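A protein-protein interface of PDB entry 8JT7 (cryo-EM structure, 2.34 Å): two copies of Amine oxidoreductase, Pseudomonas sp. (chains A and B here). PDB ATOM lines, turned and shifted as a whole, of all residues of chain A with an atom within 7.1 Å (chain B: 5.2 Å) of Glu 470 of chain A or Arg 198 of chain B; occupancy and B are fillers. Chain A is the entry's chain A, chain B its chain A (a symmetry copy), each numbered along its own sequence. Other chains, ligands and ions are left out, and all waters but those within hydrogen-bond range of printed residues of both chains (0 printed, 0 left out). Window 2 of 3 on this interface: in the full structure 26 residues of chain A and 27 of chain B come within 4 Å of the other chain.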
ATOM      1  N   GLN A 367      -2.140  -5.073 -22.938  1.00  0.00           N
ATOM      2  CA  GLN A 367      -2.735  -5.274 -21.623  1.00  0.00           C
ATOM      3  C   GLN A 367      -1.978  -4.496 -20.563  1.00  0.00           C
ATOM      4  O   GLN A 367      -2.253  -4.643 -19.383  1.00  0.00           O
ATOM      5  CB  GLN A 367      -2.707  -6.776 -21.337  1.00  0.00           C
ATOM      6  CG  GLN A 367      -3.340  -7.581 -22.478  1.00  0.00           C
ATOM      7  CD  GLN A 367      -3.730  -9.003 -22.156  1.00  0.00           C
ATOM      8  OE1 GLN A 367      -3.765  -9.426 -20.995  1.00  0.00           O
ATOM      9  NE2 GLN A 367      -4.112  -9.732 -23.195  1.00  0.00           N
ATOM     10  N   GLN A 459      -1.822 -22.772 -23.508  1.00  0.00           N
ATOM     11  CA  GLN A 459      -2.477 -21.598 -24.071  1.00  0.00           C
ATOM     12  C   GLN A 459      -3.749 -21.268 -23.294  1.00  0.00           C
ATOM     13  O   GLN A 459      -4.062 -20.094 -23.044  1.00  0.00           O
ATOM     14  CB  GLN A 459      -2.678 -21.815 -25.569  1.00  0.00           C
ATOM     15  CG  GLN A 459      -3.409 -20.707 -26.281  1.00  0.00           C
ATOM     16  CD  GLN A 459      -2.576 -19.488 -26.607  1.00  0.00           C
ATOM     17  OE1 GLN A 459      -1.433 -19.322 -26.205  1.00  0.00           O
ATOM     18  NE2 GLN A 459      -3.177 -18.591 -27.361  1.00  0.00           N
ATOM     19  N   THR A 463      -4.325 -17.739 -21.273  1.00  0.00           N
ATOM     20  CA  THR A 463      -5.531 -16.996 -21.562  1.00  0.00           C
ATOM     21  C   THR A 463      -6.274 -16.694 -20.283  1.00  0.00           C
ATOM     22  O   THR A 463      -6.657 -15.546 -20.061  1.00  0.00           O
ATOM     23  CB  THR A 463      -6.437 -17.780 -22.518  1.00  0.00           C
ATOM     24  OG1 THR A 463      -5.619 -18.153 -23.626  1.00  0.00           O
ATOM     25  CG2 THR A 463      -7.657 -17.009 -22.965  1.00  0.00           C
ATOM     26  N   ASP A 467      -6.997 -12.976 -18.326  1.00  0.00           N
ATOM     27  CA  ASP A 467      -8.392 -12.581 -18.290  1.00  0.00           C
ATOM     28  C   ASP A 467      -8.908 -12.297 -19.703  1.00  0.00           C
ATOM     29  O   ASP A 467      -9.672 -11.383 -19.925  1.00  0.00           O
ATOM     30  CB  ASP A 467      -8.607 -11.386 -17.371  1.00  0.00           C
ATOM     31  CG  ASP A 467     -10.075 -11.112 -17.064  1.00  0.00           C
ATOM     32  OD1 ASP A 467     -10.829 -12.103 -16.832  1.00  0.00           O
ATOM     33  OD2 ASP A 467     -10.470  -9.893 -17.085  1.00  0.00           O
ATOM     34  N   GLN A 468      -8.532 -13.130 -20.651  1.00  0.00           N
ATOM     35  CA  GLN A 468      -8.983 -12.978 -22.010  1.00  0.00           C
ATOM     36  C   GLN A 468      -9.947 -14.117 -22.366  1.00  0.00           C
ATOM     37  O   GLN A 468     -10.026 -15.105 -21.659  1.00  0.00           O
ATOM     38  CB  GLN A 468      -7.745 -13.020 -22.896  1.00  0.00           C
ATOM     39  CG  GLN A 468      -6.690 -12.038 -22.446  1.00  0.00           C
ATOM     40  CD  GLN A 468      -7.192 -10.653 -22.701  1.00  0.00           C
ATOM     41  OE1 GLN A 468      -7.393 -10.295 -23.852  1.00  0.00           O
ATOM     42  NE2 GLN A 468      -7.391  -9.878 -21.640  1.00  0.00           N
ATOM     43  N   ILE A 469     -10.719 -13.923 -23.432  1.00  0.00           N
ATOM     44  CA  ILE A 469     -11.545 -14.959 -23.999  1.00  0.00           C
ATOM     45  C   ILE A 469     -10.668 -15.769 -24.926  1.00  0.00           C
ATOM     46  O   ILE A 469     -10.709 -17.008 -24.902  1.00  0.00           O
ATOM     47  CB  ILE A 469     -12.777 -14.391 -24.734  1.00  0.00           C
ATOM     48  CG1 ILE A 469     -13.723 -13.750 -23.730  1.00  0.00           C
ATOM     49  CG2 ILE A 469     -13.451 -15.447 -25.584  1.00  0.00           C
ATOM     50  CD1 ILE A 469     -13.922 -12.317 -23.987  1.00  0.00           C
ATOM     51  N   GLU A 470      -9.896 -15.089 -25.743  1.00  0.00           N
ATOM     52  CA  GLU A 470      -9.126 -15.817 -26.727  1.00  0.00           C
ATOM     53  C   GLU A 470      -7.907 -15.010 -27.111  1.00  0.00           C
ATOM     54  O   GLU A 470      -8.014 -13.829 -27.416  1.00  0.00           O
ATOM     55  CB  GLU A 470      -9.986 -16.070 -27.952  1.00  0.00           C
ATOM     56  CG  GLU A 470      -9.395 -17.053 -28.940  1.00  0.00           C
ATOM     57  CD  GLU A 470     -10.352 -17.380 -30.085  1.00  0.00           C
ATOM     58  OE1 GLU A 470     -11.549 -16.909 -30.072  1.00  0.00           O
ATOM     59  OE2 GLU A 470      -9.913 -18.115 -30.995  1.00  0.00           O
ATOM     60  N   LEU A 471      -6.769 -15.670 -27.096  1.00  0.00           N
ATOM     61  CA  LEU A 471      -5.541 -15.019 -27.484  1.00  0.00           C
ATOM     62  C   LEU A 471      -5.164 -15.572 -28.843  1.00  0.00           C
ATOM     63  O   LEU A 471      -5.616 -16.637 -29.240  1.00  0.00           O
ATOM     64  CB  LEU A 471      -4.476 -15.313 -26.429  1.00  0.00           C
ATOM     65  CG  LEU A 471      -4.663 -14.593 -25.094  1.00  0.00           C
ATOM     66  CD1 LEU A 471      -3.646 -15.134 -24.120  1.00  0.00           C
ATOM     67  CD2 LEU A 471      -4.520 -13.085 -25.234  1.00  0.00           C
ATOM     68  N   PRO A 472      -4.303 -14.865 -29.587  1.00  0.00           N
ATOM     69  CA  PRO A 472      -3.748 -15.420 -30.814  1.00  0.00           C
ATOM     70  C   PRO A 472      -3.024 -16.729 -30.515  1.00  0.00           C
ATOM     71  O   PRO A 472      -2.352 -16.834 -29.509  1.00  0.00           O
ATOM     72  CB  PRO A 472      -2.736 -14.377 -31.222  1.00  0.00           C
ATOM     73  CG  PRO A 472      -3.074 -13.135 -30.468  1.00  0.00           C
ATOM     74  CD  PRO A 472      -3.690 -13.597 -29.184  1.00  0.00           C
ATOM     75  N   ALA A 473      -3.095 -17.709 -31.400  1.00  0.00           N
ATOM     76  CA  ALA A 473      -2.412 -18.962 -31.158  1.00  0.00           C
ATOM     77  C   ALA A 473      -0.891 -18.834 -31.380  1.00  0.00           C
ATOM     78  O   ALA A 473      -0.412 -18.154 -32.272  1.00  0.00           O
ATOM     79  CB  ALA A 473      -2.977 -20.002 -32.055  1.00  0.00           C
ATOM     80  N   PHE B 183      -7.106 -14.629 -35.764  1.00  0.00           N
ATOM     81  CA  PHE B 183      -7.642 -15.968 -35.511  1.00  0.00           C
ATOM     82  C   PHE B 183      -7.770 -16.742 -36.820  1.00  0.00           C
ATOM     83  O   PHE B 183      -8.757 -17.439 -37.018  1.00  0.00           O
ATOM     84  CB  PHE B 183      -8.995 -15.934 -34.786  1.00  0.00           C
ATOM     85  CG  PHE B 183      -8.951 -15.137 -33.512  1.00  0.00           C
ATOM     86  CD1 PHE B 183      -8.060 -15.470 -32.509  1.00  0.00           C
ATOM     87  CD2 PHE B 183      -9.749 -14.020 -33.338  1.00  0.00           C
ATOM     88  CE1 PHE B 183      -7.971 -14.707 -31.356  1.00  0.00           C
ATOM     89  CE2 PHE B 183      -9.615 -13.228 -32.210  1.00  0.00           C
ATOM     90  CZ  PHE B 183      -8.747 -13.592 -31.211  1.00  0.00           C
ATOM     91  N   TYR B 190     -14.647 -10.703 -41.362  1.00  0.00           N
ATOM     92  CA  TYR B 190     -15.496 -10.720 -40.190  1.00  0.00           C
ATOM     93  C   TYR B 190     -16.477  -9.558 -40.188  1.00  0.00           C
ATOM     94  O   TYR B 190     -16.138  -8.458 -40.573  1.00  0.00           O
ATOM     95  CB  TYR B 190     -14.674 -10.483 -38.920  1.00  0.00           C
ATOM     96  CG  TYR B 190     -13.764 -11.584 -38.494  1.00  0.00           C
ATOM     97  CD1 TYR B 190     -14.207 -12.522 -37.561  1.00  0.00           C
ATOM     98  CD2 TYR B 190     -12.427 -11.615 -38.906  1.00  0.00           C
ATOM     99  CE1 TYR B 190     -13.348 -13.510 -37.086  1.00  0.00           C
ATOM    100  CE2 TYR B 190     -11.569 -12.608 -38.454  1.00  0.00           C
ATOM    101  CZ  TYR B 190     -12.037 -13.549 -37.531  1.00  0.00           C
ATOM    102  OH  TYR B 190     -11.226 -14.551 -37.052  1.00  0.00           O
ATOM    103  N   ASP B 194     -19.204 -10.302 -34.828  1.00  0.00           N
ATOM    104  CA  ASP B 194     -18.565 -11.594 -34.741  1.00  0.00           C
ATOM    105  C   ASP B 194     -17.141 -11.481 -34.236  1.00  0.00           C
ATOM    106  O   ASP B 194     -16.659 -12.390 -33.573  1.00  0.00           O
ATOM    107  CB  ASP B 194     -18.382 -12.293 -36.094  1.00  0.00           C
ATOM    108  CG  ASP B 194     -19.644 -12.336 -36.900  1.00  0.00           C
ATOM    109  OD1 ASP B 194     -20.679 -12.800 -36.329  1.00  0.00           O
ATOM    110  OD2 ASP B 194     -19.585 -11.893 -38.074  1.00  0.00           O
ATOM    111  N   LEU B 195     -16.387 -10.507 -34.732  1.00  0.00           N
ATOM    112  CA  LEU B 195     -15.023 -10.376 -34.276  1.00  0.00           C
ATOM    113  C   LEU B 195     -15.024  -9.979 -32.793  1.00  0.00           C
ATOM    114  O   LEU B 195     -14.246 -10.493 -32.023  1.00  0.00           O
ATOM    115  CB  LEU B 195     -14.295  -9.342 -35.130  1.00  0.00           C
ATOM    116  CG  LEU B 195     -12.834  -9.122 -34.782  1.00  0.00           C
ATOM    117  CD1 LEU B 195     -12.113 -10.473 -34.652  1.00  0.00           C
ATOM    118  CD2 LEU B 195     -12.160  -8.249 -35.826  1.00  0.00           C
ATOM    119  N   LEU B 196     -15.861  -9.035 -32.373  1.00  0.00           N
ATOM    120  CA  LEU B 196     -15.839  -8.635 -30.979  1.00  0.00           C
ATOM    121  C   LEU B 196     -16.218  -9.788 -30.060  1.00  0.00           C
ATOM    122  O   LEU B 196     -15.745  -9.821 -28.916  1.00  0.00           O
ATOM    123  CB  LEU B 196     -16.820  -7.503 -30.704  1.00  0.00           C
ATOM    124  CG  LEU B 196     -16.416  -6.144 -31.236  1.00  0.00           C
ATOM    125  CD1 LEU B 196     -17.442  -5.113 -30.838  1.00  0.00           C
ATOM    126  CD2 LEU B 196     -15.072  -5.743 -30.744  1.00  0.00           C
ATOM    127  N   TYR B 197     -17.084 -10.685 -30.528  1.00  0.00           N
ATOM    128  CA  TYR B 197     -17.553 -11.793 -29.711  1.00  0.00           C
ATOM    129  C   TYR B 197     -16.375 -12.638 -29.256  1.00  0.00           C
ATOM    130  O   TYR B 197     -16.383 -13.162 -28.130  1.00  0.00           O
ATOM    131  CB  TYR B 197     -18.568 -12.664 -30.442  1.00  0.00           C
ATOM    132  CG  TYR B 197     -18.963 -13.859 -29.621  1.00  0.00           C
ATOM    133  CD1 TYR B 197     -19.736 -13.704 -28.493  1.00  0.00           C
ATOM    134  CD2 TYR B 197     -18.455 -15.114 -29.892  1.00  0.00           C
ATOM    135  CE1 TYR B 197     -20.054 -14.779 -27.691  1.00  0.00           C
ATOM    136  CE2 TYR B 197     -18.776 -16.205 -29.107  1.00  0.00           C
ATOM    137  CZ  TYR B 197     -19.586 -16.035 -28.006  1.00  0.00           C
ATOM    138  OH  TYR B 197     -19.881 -17.079 -27.142  1.00  0.00           O
ATOM    139  N   ARG B 198     -15.333 -12.680 -30.089  1.00  0.00           N
ATOM    140  CA  ARG B 198     -14.146 -13.469 -29.808  1.00  0.00           C
ATOM    141  C   ARG B 198     -13.216 -12.814 -28.801  1.00  0.00           C
ATOM    142  O   ARG B 198     -12.438 -13.529 -28.188  1.00  0.00           O
ATOM    143  CB  ARG B 198     -13.410 -13.773 -31.113  1.00  0.00           C
ATOM    144  CG  ARG B 198     -14.337 -14.557 -32.026  1.00  0.00           C
ATOM    145  CD  ARG B 198     -13.671 -15.321 -33.115  1.00  0.00           C
ATOM    146  NE  ARG B 198     -12.948 -16.439 -32.555  1.00  0.00           N
ATOM    147  CZ  ARG B 198     -12.236 -17.257 -33.296  1.00  0.00           C
ATOM    148  NH1 ARG B 198     -12.353 -17.188 -34.612  1.00  0.00           N
ATOM    149  NH2 ARG B 198     -11.456 -18.154 -32.725  1.00  0.00           N
ATOM    150  N   VAL B 199     -13.266 -11.493 -28.617  1.00  0.00           N
ATOM    151  CA  VAL B 199     -12.246 -10.852 -27.790  1.00  0.00           C
ATOM    152  C   VAL B 199     -12.855 -10.149 -26.580  1.00  0.00           C
ATOM    153  O   VAL B 199     -12.175  -9.882 -25.613  1.00  0.00           O
ATOM    154  CB  VAL B 199     -11.384  -9.918 -28.650  1.00  0.00           C
ATOM    155  CG1 VAL B 199     -10.638 -10.762 -29.676  1.00  0.00           C
ATOM    156  CG2 VAL B 199     -12.192  -8.849 -29.341  1.00  0.00           C
ATOM    157  N   LEU B 200     -14.158  -9.930 -26.592  1.00  0.00           N
ATOM    158  CA  LEU B 200     -14.752  -9.058 -25.613  1.00  0.00           C
ATOM    159  C   LEU B 200     -15.895  -9.835 -25.005  1.00  0.00           C
ATOM    160  O   LEU B 200     -16.478 -10.667 -25.690  1.00  0.00           O
ATOM    161  CB  LEU B 200     -15.136  -7.798 -26.383  1.00  0.00           C
ATOM    162  CG  LEU B 200     -15.760  -6.665 -25.604  1.00  0.00           C
ATOM    163  CD1 LEU B 200     -14.708  -5.952 -24.760  1.00  0.00           C
ATOM    164  CD2 LEU B 200     -16.453  -5.712 -26.568  1.00  0.00           C
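The guanidinium group (NE) of Arg 198 of chain B is in salt-bridge range of the side-chain carboxylate (OE1) of Glu 470 of chain A, at 2.9 Å.
No position is printed for both chains.
Among the printed residues, pairs that only touch across the chains: Ile 469 of chain A with Leu 200 of chain B (3.3 Å), Ile 469 of chain A with Arg 198 of chain B (3.4 Å), Ile 469 of chain A with Val 199 of chain B (3.4 Å), Glu 470 of chain A with Phe 183 of chain B (3.6 Å) and Leu 471 of chain A with Phe 183 of chain B (3.7 Å).
Of the 10 printed residues of chain A, 3 touch a printed residue of chain B.
Printed residues of chain B that touch a printed residue of chain A: Phe 183, Arg 198, Val 199 and Leu 200.
Hydrophobic or aromatic side chains of chain B within 4 Å of the printed part of chain A: Phe 183.
Among the printed residues, 6 pairs touch across the chains.
Among the printed residues, Asp or Glu carboxylates within 4 Å of a Lys or Arg side-chain nitrogen of the other chain: Glu 470 of chain A with Arg 198 of chain B.
Of the printed residues of chain B, Ile 469 of chain A touches Arg 198, Val 199 and Leu 200.
Of chain B, only Phe 183 (3.6 Å) and Arg 198 (2.3 Å) come within 4 Å of Glu 470 of chain A.
Of the printed residues of chain B, Leu 471 of chain A touches Phe 183.
Ala 473 of chain A touches none of the printed residues of chain B.
Printed residues of chain A within 4 Å of Phe 183 of chain B: Glu 470 (3.6 Å) and Leu 471 (3.7 Å).
Arg 198 of chain B touches two residues of chain A.
Of the printed residues of chain A, Val 199 of chain B touches Ile 469 (3.4 Å).
Of the printed residues of chain A, Leu 200 of chain B touches Ile 469.
The nearest printed residue of chain B that does not touch Leu 471 of chain A is Arg 198 of chain B (6.2 Å).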
